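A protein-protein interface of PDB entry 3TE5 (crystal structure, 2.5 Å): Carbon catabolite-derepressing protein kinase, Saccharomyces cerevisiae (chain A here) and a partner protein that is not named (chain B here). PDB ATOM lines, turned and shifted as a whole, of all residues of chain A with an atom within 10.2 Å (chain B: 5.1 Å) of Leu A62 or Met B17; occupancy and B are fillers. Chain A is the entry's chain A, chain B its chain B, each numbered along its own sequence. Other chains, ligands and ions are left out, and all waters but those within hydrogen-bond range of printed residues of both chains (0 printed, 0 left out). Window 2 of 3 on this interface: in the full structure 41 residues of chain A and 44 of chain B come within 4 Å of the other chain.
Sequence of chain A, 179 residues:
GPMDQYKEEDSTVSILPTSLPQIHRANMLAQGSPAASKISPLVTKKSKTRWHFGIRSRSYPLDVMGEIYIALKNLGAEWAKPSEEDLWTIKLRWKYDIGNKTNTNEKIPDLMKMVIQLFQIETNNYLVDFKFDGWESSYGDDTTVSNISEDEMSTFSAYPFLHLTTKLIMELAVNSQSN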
ATOM      1  N   SER A  57      19.256  -5.700   8.272  1.00  0.00           N
ATOM      2  CA  SER A  57      19.172  -7.159   8.355  1.00  0.00           C
ATOM      3  C   SER A  57      17.943  -7.704   7.635  1.00  0.00           C
ATOM      4  O   SER A  57      16.850  -7.127   7.713  1.00  0.00           O
ATOM      5  CB  SER A  57      19.181  -7.626   9.813  1.00  0.00           C
ATOM      6  OG  SER A  57      19.402  -9.024   9.900  1.00  0.00           O
ATOM      7  N   ARG A  58      18.140  -8.821   6.939  1.00  0.00           N
ATOM      8  CA  ARG A  58      17.068  -9.496   6.207  1.00  0.00           C
ATOM      9  C   ARG A  58      16.348 -10.568   7.032  1.00  0.00           C
ATOM     10  O   ARG A  58      15.255 -11.005   6.668  1.00  0.00           O
ATOM     11  CB  ARG A  58      17.594 -10.089   4.894  1.00  0.00           C
ATOM     12  CG  ARG A  58      17.829  -9.058   3.794  1.00  0.00           C
ATOM     13  CD  ARG A  58      16.565  -8.249   3.508  1.00  0.00           C
ATOM     14  NE  ARG A  58      16.791  -7.202   2.515  1.00  0.00           N
ATOM     15  CZ  ARG A  58      16.214  -7.161   1.318  1.00  0.00           C
ATOM     16  NH1 ARG A  58      15.356  -8.109   0.952  1.00  0.00           N
ATOM     17  NH2 ARG A  58      16.489  -6.165   0.485  1.00  0.00           N
ATOM     18  N   SER A  59      16.958 -10.981   8.143  1.00  0.00           N
ATOM     19  CA  SER A  59      16.327 -11.917   9.074  1.00  0.00           C
ATOM     20  C   SER A  59      15.145 -11.265   9.797  1.00  0.00           C
ATOM     21  O   SER A  59      14.830 -10.096   9.561  1.00  0.00           O
ATOM     22  CB  SER A  59      17.349 -12.447  10.080  1.00  0.00           C
ATOM     23  OG  SER A  59      18.442 -13.046   9.410  1.00  0.00           O
ATOM     24  N   TYR A  60      14.494 -12.019  10.677  1.00  0.00           N
ATOM     25  CA  TYR A  60      13.290 -11.540  11.350  1.00  0.00           C
ATOM     26  C   TYR A  60      13.540 -11.166  12.821  1.00  0.00           C
ATOM     27  O   TYR A  60      14.543 -11.590  13.400  1.00  0.00           O
ATOM     28  CB  TYR A  60      12.159 -12.557  11.178  1.00  0.00           C
ATOM     29  CG  TYR A  60      11.721 -12.708   9.736  1.00  0.00           C
ATOM     30  CD1 TYR A  60      10.841 -11.793   9.156  1.00  0.00           C
ATOM     31  CD2 TYR A  60      12.196 -13.755   8.947  1.00  0.00           C
ATOM     32  CE1 TYR A  60      10.440 -11.920   7.826  1.00  0.00           C
ATOM     33  CE2 TYR A  60      11.798 -13.892   7.616  1.00  0.00           C
ATOM     34  CZ  TYR A  60      10.920 -12.973   7.065  1.00  0.00           C
ATOM     35  OH  TYR A  60      10.525 -13.099   5.753  1.00  0.00           O
ATOM     36  N   PRO A  61      12.639 -10.357  13.419  1.00  0.00           N
ATOM     37  CA  PRO A  61      12.878  -9.690  14.705  1.00  0.00           C
ATOM     38  C   PRO A  61      13.559 -10.524  15.798  1.00  0.00           C
ATOM     39  O   PRO A  61      14.658 -10.168  16.232  1.00  0.00           O
ATOM     40  CB  PRO A  61      11.477  -9.253  15.131  1.00  0.00           C
ATOM     41  CG  PRO A  61      10.793  -8.983  13.861  1.00  0.00           C
ATOM     42  CD  PRO A  61      11.318  -9.993  12.874  1.00  0.00           C
ATOM     43  N   LEU A  62      12.921 -11.613  16.228  1.00  0.00           N
ATOM     44  CA  LEU A  62      13.439 -12.455  17.313  1.00  0.00           C
ATOM     45  C   LEU A  62      14.775 -13.097  16.955  1.00  0.00           C
ATOM     46  O   LEU A  62      15.654 -13.236  17.810  1.00  0.00           O
ATOM     47  CB  LEU A  62      12.421 -13.539  17.690  1.00  0.00           C
ATOM     48  CG  LEU A  62      11.070 -13.080  18.254  1.00  0.00           C
ATOM     49  CD1 LEU A  62       9.962 -14.067  17.894  1.00  0.00           C
ATOM     50  CD2 LEU A  62      11.144 -12.857  19.761  1.00  0.00           C
ATOM     51  N   ASP A  63      14.912 -13.484  15.688  1.00  0.00           N
ATOM     52  CA  ASP A  63      16.155 -14.033  15.157  1.00  0.00           C
ATOM     53  C   ASP A  63      17.275 -12.993  15.250  1.00  0.00           C
ATOM     54  O   ASP A  63      18.348 -13.276  15.792  1.00  0.00           O
ATOM     55  CB  ASP A  63      15.949 -14.493  13.706  1.00  0.00           C
ATOM     56  CG  ASP A  63      17.142 -15.247  13.142  1.00  0.00           C
ATOM     57  OD1 ASP A  63      17.976 -15.746  13.924  1.00  0.00           O
ATOM     58  OD2 ASP A  63      17.238 -15.348  11.900  1.00  0.00           O
ATOM     59  N   VAL A  64      17.004 -11.792  14.739  1.00  0.00           N
ATOM     60  CA  VAL A  64      17.953 -10.681  14.778  1.00  0.00           C
ATOM     61  C   VAL A  64      18.325 -10.326  16.219  1.00  0.00           C
ATOM     62  O   VAL A  64      19.513 -10.196  16.541  1.00  0.00           O
ATOM     63  CB  VAL A  64      17.410  -9.430  14.036  1.00  0.00           C
ATOM     64  CG1 VAL A  64      18.310  -8.219  14.266  1.00  0.00           C
ATOM     65  CG2 VAL A  64      17.285  -9.706  12.549  1.00  0.00           C
ATOM     66  N   MET A  65      17.315 -10.185  17.078  1.00  0.00           N
ATOM     67  CA  MET A  65      17.539  -9.844  18.484  1.00  0.00           C
ATOM     68  C   MET A  65      18.336 -10.936  19.192  1.00  0.00           C
ATOM     69  O   MET A  65      19.152 -10.646  20.069  1.00  0.00           O
ATOM     70  CB  MET A  65      16.218  -9.591  19.213  1.00  0.00           C
ATOM     71  CG  MET A  65      15.423  -8.385  18.718  1.00  0.00           C
ATOM     72  SD  MET A  65      16.189  -6.772  19.008  1.00  0.00           S
ATOM     73  CE  MET A  65      16.042  -6.627  20.787  1.00  0.00           C
ATOM     74  N   GLY A  66      18.095 -12.184  18.798  1.00  0.00           N
ATOM     75  CA  GLY A  66      18.867 -13.321  19.293  1.00  0.00           C
ATOM     76  C   GLY A  66      20.334 -13.208  18.924  1.00  0.00           C
ATOM     77  O   GLY A  66      21.208 -13.359  19.779  1.00  0.00           O
ATOM     78  N   GLU A  67      20.595 -12.926  17.649  1.00  0.00           N
ATOM     79  CA  GLU A  67      21.961 -12.738  17.142  1.00  0.00           C
ATOM     80  C   GLU A  67      22.730 -11.650  17.898  1.00  0.00           C
ATOM     81  O   GLU A  67      23.894 -11.845  18.259  1.00  0.00           O
ATOM     82  CB  GLU A  67      21.948 -12.420  15.643  1.00  0.00           C
ATOM     83  CG  GLU A  67      21.673 -13.619  14.740  1.00  0.00           C
ATOM     84  CD  GLU A  67      21.794 -13.286  13.256  1.00  0.00           C
ATOM     85  OE1 GLU A  67      22.337 -14.126  12.503  1.00  0.00           O
ATOM     86  OE2 GLU A  67      21.353 -12.188  12.841  1.00  0.00           O
ATOM     87  N   ILE A  68      22.071 -10.519  18.141  1.00  0.00           N
ATOM     88  CA  ILE A  68      22.698  -9.378  18.810  1.00  0.00           C
ATOM     89  C   ILE A  68      23.144  -9.724  20.235  1.00  0.00           C
ATOM     90  O   ILE A  68      24.287  -9.449  20.613  1.00  0.00           O
ATOM     91  CB  ILE A  68      21.783  -8.119  18.790  1.00  0.00           C
ATOM     92  CG1 ILE A  68      21.521  -7.677  17.348  1.00  0.00           C
ATOM     93  CG2 ILE A  68      22.409  -6.971  19.582  1.00  0.00           C
ATOM     94  CD1 ILE A  68      20.342  -6.742  17.186  1.00  0.00           C
ATOM     95  N   TYR A  69      22.246 -10.341  21.006  1.00  0.00           N
ATOM     96  CA  TYR A  69      22.531 -10.732  22.385  1.00  0.00           C
ATOM     97  C   TYR A  69      23.699 -11.711  22.504  1.00  0.00           C
ATOM     98  O   TYR A  69      24.534 -11.577  23.404  1.00  0.00           O
ATOM     99  CB  TYR A  69      21.281 -11.302  23.062  1.00  0.00           C
ATOM    100  CG  TYR A  69      20.392 -10.247  23.682  1.00  0.00           C
ATOM    101  CD1 TYR A  69      20.754  -9.623  24.875  1.00  0.00           C
ATOM    102  CD2 TYR A  69      19.194  -9.872  23.080  1.00  0.00           C
ATOM    103  CE1 TYR A  69      19.950  -8.650  25.451  1.00  0.00           C
ATOM    104  CE2 TYR A  69      18.380  -8.898  23.650  1.00  0.00           C
ATOM    105  CZ  TYR A  69      18.765  -8.295  24.836  1.00  0.00           C
ATOM    106  OH  TYR A  69      17.968  -7.333  25.412  1.00  0.00           O
ATOM    107  N   ILE A  70      23.755 -12.682  21.592  1.00  0.00           N
ATOM    108  CA  ILE A  70      24.863 -13.641  21.535  1.00  0.00           C
ATOM    109  C   ILE A  70      26.192 -12.910  21.339  1.00  0.00           C
ATOM    110  O   ILE A  70      27.170 -13.182  22.043  1.00  0.00           O
ATOM    111  CB  ILE A  70      24.649 -14.714  20.427  1.00  0.00           C
ATOM    112  CG1 ILE A  70      23.425 -15.580  20.751  1.00  0.00           C
ATOM    113  CG2 ILE A  70      25.902 -15.586  20.260  1.00  0.00           C
ATOM    114  CD1 ILE A  70      22.999 -16.532  19.636  1.00  0.00           C
ATOM    115  N   PRO A  82      14.401  -6.380  29.792  1.00  0.00           N
ATOM    116  CA  PRO A  82      13.389  -5.601  29.081  1.00  0.00           C
ATOM    117  C   PRO A  82      11.959  -5.980  29.464  1.00  0.00           C
ATOM    118  O   PRO A  82      11.679  -7.138  29.786  1.00  0.00           O
ATOM    119  CB  PRO A  82      13.654  -5.942  27.612  1.00  0.00           C
ATOM    120  CG  PRO A  82      14.256  -7.290  27.637  1.00  0.00           C
ATOM    121  CD  PRO A  82      15.000  -7.422  28.937  1.00  0.00           C
ATOM    122  N   SER A  83      11.070  -4.993  29.425  1.00  0.00           N
ATOM    123  CA  SER A  83       9.659  -5.205  29.707  1.00  0.00           C
ATOM    124  C   SER A  83       8.911  -5.496  28.410  1.00  0.00           C
ATOM    125  O   SER A  83       9.508  -5.502  27.329  1.00  0.00           O
ATOM    126  CB  SER A  83       9.068  -3.977  30.401  1.00  0.00           C
ATOM    127  OG  SER A  83       9.061  -2.858  29.532  1.00  0.00           O
ATOM    128  N   GLU A  84       7.606  -5.732  28.523  1.00  0.00           N
ATOM    129  CA  GLU A  84       6.769  -6.052  27.369  1.00  0.00           C
ATOM    130  C   GLU A  84       6.687  -4.897  26.372  1.00  0.00           C
ATOM    131  O   GLU A  84       6.665  -5.122  25.164  1.00  0.00           O
ATOM    132  CB  GLU A  84       5.365  -6.469  27.820  1.00  0.00           C
ATOM    133  N   LEU A  87      10.444  -4.561  24.051  1.00  0.00           N
ATOM    134  CA  LEU A  87      11.145  -5.816  23.744  1.00  0.00           C
ATOM    135  C   LEU A  87      12.306  -5.638  22.761  1.00  0.00           C
ATOM    136  O   LEU A  87      13.318  -6.341  22.845  1.00  0.00           O
ATOM    137  CB  LEU A  87      10.169  -6.861  23.188  1.00  0.00           C
ATOM    138  CG  LEU A  87       8.928  -7.276  23.985  1.00  0.00           C
ATOM    139  CD1 LEU A  87       7.929  -7.931  23.054  1.00  0.00           C
ATOM    140  CD2 LEU A  87       9.272  -8.200  25.149  1.00  0.00           C
ATOM    141  N   TRP A  88      12.153  -4.686  21.845  1.00  0.00           N
ATOM    142  CA  TRP A  88      13.107  -4.471  20.760  1.00  0.00           C
ATOM    143  C   TRP A  88      14.135  -3.390  21.099  1.00  0.00           C
ATOM    144  O   TRP A  88      14.798  -2.840  20.214  1.00  0.00           O
ATOM    145  CB  TRP A  88      12.344  -4.143  19.479  1.00  0.00           C
ATOM    146  CG  TRP A  88      11.081  -4.939  19.379  1.00  0.00           C
ATOM    147  CD1 TRP A  88       9.809  -4.494  19.600  1.00  0.00           C
ATOM    148  CD2 TRP A  88      10.971  -6.336  19.080  1.00  0.00           C
ATOM    149  NE1 TRP A  88       8.914  -5.521  19.435  1.00  0.00           N
ATOM    150  CE2 TRP A  88       9.601  -6.662  19.117  1.00  0.00           C
ATOM    151  CE3 TRP A  88      11.898  -7.338  18.772  1.00  0.00           C
ATOM    152  CZ2 TRP A  88       9.132  -7.952  18.857  1.00  0.00           C
ATOM    153  CZ3 TRP A  88      11.433  -8.620  18.520  1.00  0.00           C
ATOM    154  CH2 TRP A  88      10.061  -8.914  18.561  1.00  0.00           C
ATOM    155  N   ILE A  90      17.474  -2.689  23.591  1.00  0.00           N
ATOM    156  CA  ILE A  90      18.491  -3.234  24.481  1.00  0.00           C
ATOM    157  C   ILE A  90      19.216  -2.095  25.188  1.00  0.00           C
ATOM    158  O   ILE A  90      19.889  -1.279  24.554  1.00  0.00           O
ATOM    159  CB  ILE A  90      19.505  -4.144  23.745  1.00  0.00           C
ATOM    160  CG1 ILE A  90      18.775  -5.221  22.934  1.00  0.00           C
ATOM    161  CG2 ILE A  90      20.475  -4.776  24.747  1.00  0.00           C
ATOM    162  CD1 ILE A  90      19.619  -5.889  21.866  1.00  0.00           C
ATOM    163  N   LEU A 118      15.714  -1.950  17.485  1.00  0.00           N
ATOM    164  CA  LEU A 118      15.327  -2.561  16.223  1.00  0.00           C
ATOM    165  C   LEU A 118      14.155  -1.801  15.612  1.00  0.00           C
ATOM    166  O   LEU A 118      13.133  -1.576  16.265  1.00  0.00           O
ATOM    167  CB  LEU A 118      14.980  -4.039  16.422  1.00  0.00           C
ATOM    168  CG  LEU A 118      14.798  -4.923  15.184  1.00  0.00           C
ATOM    169  CD1 LEU A 118      16.104  -5.087  14.416  1.00  0.00           C
ATOM    170  CD2 LEU A 118      14.254  -6.283  15.590  1.00  0.00           C
ATOM    171  N   THR A 123       8.661  -5.564   5.559  1.00  0.00           N
ATOM    172  CA  THR A 123       8.293  -6.829   6.217  1.00  0.00           C
ATOM    173  C   THR A 123       9.489  -7.770   6.385  1.00  0.00           C
ATOM    174  O   THR A 123       9.555  -8.542   7.344  1.00  0.00           O
ATOM    175  CB  THR A 123       7.146  -7.574   5.472  1.00  0.00           C
ATOM    176  OG1 THR A 123       7.654  -8.206   4.290  1.00  0.00           O
ATOM    177  CG2 THR A 123       6.010  -6.610   5.094  1.00  0.00           C
ATOM    178  N   TYR A 126      14.895  -4.955   8.159  1.00  0.00           N
ATOM    179  CA  TYR A 126      15.006  -4.357   9.489  1.00  0.00           C
ATOM    180  C   TYR A 126      16.322  -3.610   9.696  1.00  0.00           C
ATOM    181  O   TYR A 126      17.350  -3.964   9.115  1.00  0.00           O
ATOM    182  CB  TYR A 126      14.835  -5.424  10.573  1.00  0.00           C
ATOM    183  CG  TYR A 126      13.460  -6.048  10.604  1.00  0.00           C
ATOM    184  CD1 TYR A 126      12.440  -5.488  11.369  1.00  0.00           C
ATOM    185  CD2 TYR A 126      13.176  -7.206   9.871  1.00  0.00           C
ATOM    186  CE1 TYR A 126      11.170  -6.056  11.403  1.00  0.00           C
ATOM    187  CE2 TYR A 126      11.907  -7.783   9.898  1.00  0.00           C
ATOM    188  CZ  TYR A 126      10.911  -7.202  10.667  1.00  0.00           C
ATOM    189  OH  TYR A 126       9.655  -7.763  10.703  1.00  0.00           O
ATOM    190  N   VAL B  10      12.522 -14.425  25.997  1.00  0.00           N
ATOM    191  CA  VAL B  10      11.750 -14.199  24.765  1.00  0.00           C
ATOM    192  C   VAL B  10      12.536 -14.478  23.468  1.00  0.00           C
ATOM    193  O   VAL B  10      11.942 -14.811  22.443  1.00  0.00           O
ATOM    194  CB  VAL B  10      11.095 -12.774  24.752  1.00  0.00           C
ATOM    195  CG1 VAL B  10      12.152 -11.670  24.787  1.00  0.00           C
ATOM    196  CG2 VAL B  10      10.155 -12.595  23.562  1.00  0.00           C
ATOM    197  N   PHE B  11      13.862 -14.356  23.523  1.00  0.00           N
ATOM    198  CA  PHE B  11      14.709 -14.604  22.350  1.00  0.00           C
ATOM    199  C   PHE B  11      15.389 -15.982  22.364  1.00  0.00           C
ATOM    200  O   PHE B  11      16.071 -16.348  21.402  1.00  0.00           O
ATOM    201  CB  PHE B  11      15.758 -13.493  22.183  1.00  0.00           C
ATOM    202  CG  PHE B  11      15.200 -12.101  22.313  1.00  0.00           C
ATOM    203  CD1 PHE B  11      14.219 -11.641  21.439  1.00  0.00           C
ATOM    204  CD2 PHE B  11      15.662 -11.247  23.313  1.00  0.00           C
ATOM    205  CE1 PHE B  11      13.696 -10.352  21.564  1.00  0.00           C
ATOM    206  CE2 PHE B  11      15.148  -9.955  23.442  1.00  0.00           C
ATOM    207  CZ  PHE B  11      14.168  -9.508  22.565  1.00  0.00           C
ATOM    208  N   ASP B  13      13.604 -18.844  24.229  1.00  0.00           N
ATOM    209  CA  ASP B  13      12.563 -19.814  24.544  1.00  0.00           C
ATOM    210  C   ASP B  13      11.268 -19.440  23.826  1.00  0.00           C
ATOM    211  O   ASP B  13      10.658 -18.417  24.151  1.00  0.00           O
ATOM    212  CB  ASP B  13      12.342 -19.873  26.061  1.00  0.00           C
ATOM    213  CG  ASP B  13      11.371 -20.976  26.487  1.00  0.00           C
ATOM    214  OD1 ASP B  13      10.833 -21.706  25.622  1.00  0.00           O
ATOM    215  OD2 ASP B  13      11.149 -21.111  27.708  1.00  0.00           O
ATOM    216  N   PRO B  14      10.842 -20.272  22.850  1.00  0.00           N
ATOM    217  CA  PRO B  14       9.642 -20.017  22.042  1.00  0.00           C
ATOM    218  C   PRO B  14       8.352 -19.891  22.849  1.00  0.00           C
ATOM    219  O   PRO B  14       7.378 -19.326  22.358  1.00  0.00           O
ATOM    220  CB  PRO B  14       9.572 -21.244  21.129  1.00  0.00           C
ATOM    221  CG  PRO B  14      10.974 -21.713  21.028  1.00  0.00           C
ATOM    222  CD  PRO B  14      11.557 -21.477  22.388  1.00  0.00           C
ATOM    223  N   SER B  15       8.356 -20.410  24.076  1.00  0.00           N
ATOM    224  CA  SER B  15       7.181 -20.376  24.947  1.00  0.00           C
ATOM    225  C   SER B  15       6.766 -18.953  25.300  1.00  0.00           C
ATOM    226  O   SER B  15       5.574 -18.663  25.428  1.00  0.00           O
ATOM    227  CB  SER B  15       7.445 -21.157  26.238  1.00  0.00           C
ATOM    228  OG  SER B  15       7.852 -22.485  25.967  1.00  0.00           O
ATOM    229  N   VAL B  16       7.757 -18.075  25.442  1.00  0.00           N
ATOM    230  CA  VAL B  16       7.542 -16.712  25.925  1.00  0.00           C
ATOM    231  C   VAL B  16       6.758 -15.844  24.934  1.00  0.00           C
ATOM    232  O   VAL B  16       5.760 -15.227  25.309  1.00  0.00           O
ATOM    233  CB  VAL B  16       8.875 -16.039  26.342  1.00  0.00           C
ATOM    234  CG1 VAL B  16       8.622 -14.676  26.976  1.00  0.00           C
ATOM    235  CG2 VAL B  16       9.640 -16.928  27.312  1.00  0.00           C
ATOM    236  N   MET B  17       7.198 -15.807  23.676  1.00  0.00           N
ATOM    237  CA  MET B  17       6.492 -15.050  22.638  1.00  0.00           C
ATOM    238  C   MET B  17       5.156 -15.701  22.286  1.00  0.00           C
ATOM    239  O   MET B  17       4.222 -15.017  21.853  1.00  0.00           O
ATOM    240  CB  MET B  17       7.362 -14.879  21.386  1.00  0.00           C
ATOM    241  CG  MET B  17       6.799 -13.918  20.328  1.00  0.00           C
ATOM    242  SD  MET B  17       6.688 -12.194  20.868  1.00  0.00           S
ATOM    243  CE  MET B  17       6.030 -11.421  19.395  1.00  0.00           C
ATOM    244  N   GLU B  18       5.071 -17.018  22.477  1.00  0.00           N
ATOM    245  CA  GLU B  18       3.825 -17.754  22.280  1.00  0.00           C
ATOM    246  C   GLU B  18       2.758 -17.265  23.256  1.00  0.00           C
ATOM    247  O   GLU B  18       1.627 -16.989  22.853  1.00  0.00           O
ATOM    248  CB  GLU B  18       4.050 -19.261  22.426  1.00  0.00           C
ATOM    249  CG  GLU B  18       2.838 -20.115  22.057  1.00  0.00           C
ATOM    250  CD  GLU B  18       3.120 -21.610  22.094  1.00  0.00           C
ATOM    251  OE1 GLU B  18       3.727 -22.091  23.075  1.00  0.00           O
ATOM    252  OE2 GLU B  18       2.718 -22.310  21.139  1.00  0.00           O
ATOM    253  N   ARG B  19       3.129 -17.145  24.531  1.00  0.00           N
ATOM    254  CA  ARG B  19       2.227 -16.623  25.561  1.00  0.00           C
ATOM    255  C   ARG B  19       1.686 -15.241  25.206  1.00  0.00           C
ATOM    256  O   ARG B  19       0.487 -14.991  25.363  1.00  0.00           O
ATOM    257  CB  ARG B  19       2.907 -16.590  26.935  1.00  0.00           C
ATOM    258  CG  ARG B  19       2.703 -17.852  27.756  1.00  0.00           C
ATOM    259  CD  ARG B  19       3.371 -17.767  29.130  1.00  0.00           C
ATOM    260  NE  ARG B  19       4.831 -17.885  29.060  1.00  0.00           N
ATOM    261  CZ  ARG B  19       5.501 -19.038  29.014  1.00  0.00           C
ATOM    262  NH1 ARG B  19       4.859 -20.200  29.023  1.00  0.00           N
ATOM    263  NH2 ARG B  19       6.829 -19.026  28.952  1.00  0.00           N
ATOM    264  N   TYR B  20       2.566 -14.362  24.721  1.00  0.00           N
ATOM    265  CA  TYR B  20       2.171 -13.016  24.301  1.00  0.00           C
ATOM    266  C   TYR B  20       1.136 -13.052  23.179  1.00  0.00           C
ATOM    267  O   TYR B  20       0.105 -12.381  23.270  1.00  0.00           O
ATOM    268  CB  TYR B  20       3.383 -12.181  23.863  1.00  0.00           C
ATOM    269  CG  TYR B  20       4.440 -11.950  24.923  1.00  0.00           C
ATOM    270  CD1 TYR B  20       4.092 -11.667  26.246  1.00  0.00           C
ATOM    271  CD2 TYR B  20       5.794 -11.984  24.592  1.00  0.00           C
ATOM    272  CE1 TYR B  20       5.071 -11.449  27.217  1.00  0.00           C
ATOM    273  CE2 TYR B  20       6.779 -11.764  25.551  1.00  0.00           C
ATOM    274  CZ  TYR B  20       6.412 -11.496  26.861  1.00  0.00           C
ATOM    275  OH  TYR B  20       7.389 -11.278  27.810  1.00  0.00           O
ATOM    276  N   TYR B  21       1.412 -13.836  22.133  1.00  0.00           N
ATOM    277  CA  TYR B  21       0.490 -13.985  21.002  1.00  0.00           C
ATOM    278  C   TYR B  21      -0.901 -14.427  21.452  1.00  0.00           C
ATOM    279  O   TYR B  21      -1.907 -13.916  20.960  1.00  0.00           O
ATOM    280  CB  TYR B  21       1.021 -14.995  19.972  1.00  0.00           C
ATOM    281  CG  TYR B  21       2.111 -14.499  19.035  1.00  0.00           C
ATOM    282  CD1 TYR B  21       2.004 -13.268  18.380  1.00  0.00           C
ATOM    283  CD2 TYR B  21       3.233 -15.289  18.767  1.00  0.00           C
ATOM    284  CE1 TYR B  21       3.003 -12.824  17.510  1.00  0.00           C
ATOM    285  CE2 TYR B  21       4.234 -14.857  17.897  1.00  0.00           C
ATOM    286  CZ  TYR B  21       4.114 -13.625  17.273  1.00  0.00           C
ATOM    287  OH  TYR B  21       5.102 -13.197  16.414  1.00  0.00           O
ATOM    288  N   LEU B  36       4.052  -6.102  19.741  1.00  0.00           N
ATOM    289  CA  LEU B  36       4.490  -7.454  19.375  1.00  0.00           C
ATOM    290  C   LEU B  36       5.465  -7.432  18.198  1.00  0.00           C
ATOM    291  O   LEU B  36       6.141  -8.424  17.916  1.00  0.00           O
ATOM    292  CB  LEU B  36       3.286  -8.348  19.052  1.00  0.00           C
ATOM    293  CG  LEU B  36       2.270  -8.645  20.165  1.00  0.00           C
ATOM    294  CD1 LEU B  36       0.986  -9.214  19.577  1.00  0.00           C
ATOM    295  CD2 LEU B  36       2.840  -9.582  21.225  1.00  0.00           C
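The backbone carbonyl oxygen (O) of Trp A88 is in hydrogen-bond range of the backbone NH (N) of Leu A118.
O of Val B10 touches CD2 of Leu A62, 3.4 Å away.
Leu A62 touches Phe B11 (CD2 to CD1, 3.7 Å).
CD1 of Leu A62 touches CG of Met B17, 3.99 Å away.
CB of Met A65 touches CE1 of Phe B11, 3.5 Å away.
CE2 of Tyr A69 touches CE2 of Phe B11, 3.4 Å away.
Leu A87 touches Phe B11.
Leu B36 touches Trp A88 (O to CZ2, 3.2 Å).
Printed residues of chain B within 4 Å of Leu A62: Val B10 (3.4 Å), Phe B11 (3.7 Å) and Met B17 (3.99 Å).
Of the printed residues of chain A, Met B17 touches Leu A62 (3.99 Å).
Val B10 touches one residue of chain A.
No residue of chain A comes within 4 Å of Val B16.
No residue of chain A comes within 4 Å of Tyr B20.
Of the printed residues of chain A, Leu B36 touches Trp A88.
Of the printed residues of chain B, Tyr A69 touches Phe B11.
Printed residues of chain B within 4 Å of Leu A87: Phe B11.
Of the printed residues of chain B, Trp A88 touches Leu B36.
Of the printed residues of chain A, Phe B11 touches Leu A62 (3.7 Å), Met A65 (3.5 Å), Tyr A69 (3.4 Å) and Leu A87 (3.3 Å).
Of the printed residues of chain B, Met A65 touches Phe B11 (3.5 Å).
Of the 23 printed residues of chain A, 5 touch a printed residue of chain B.
Hydrophobic or aromatic side chains of chain A within 4 Å of the printed part of chain B: Leu A62, Met A65, Tyr A69 and Trp A88.
Among the printed residues, 7 pairs touch across the chains.
Among the printed residues, no Asp or Glu carboxylate lies within 4 Å of a Lys or Arg side-chain nitrogen of the other chain.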
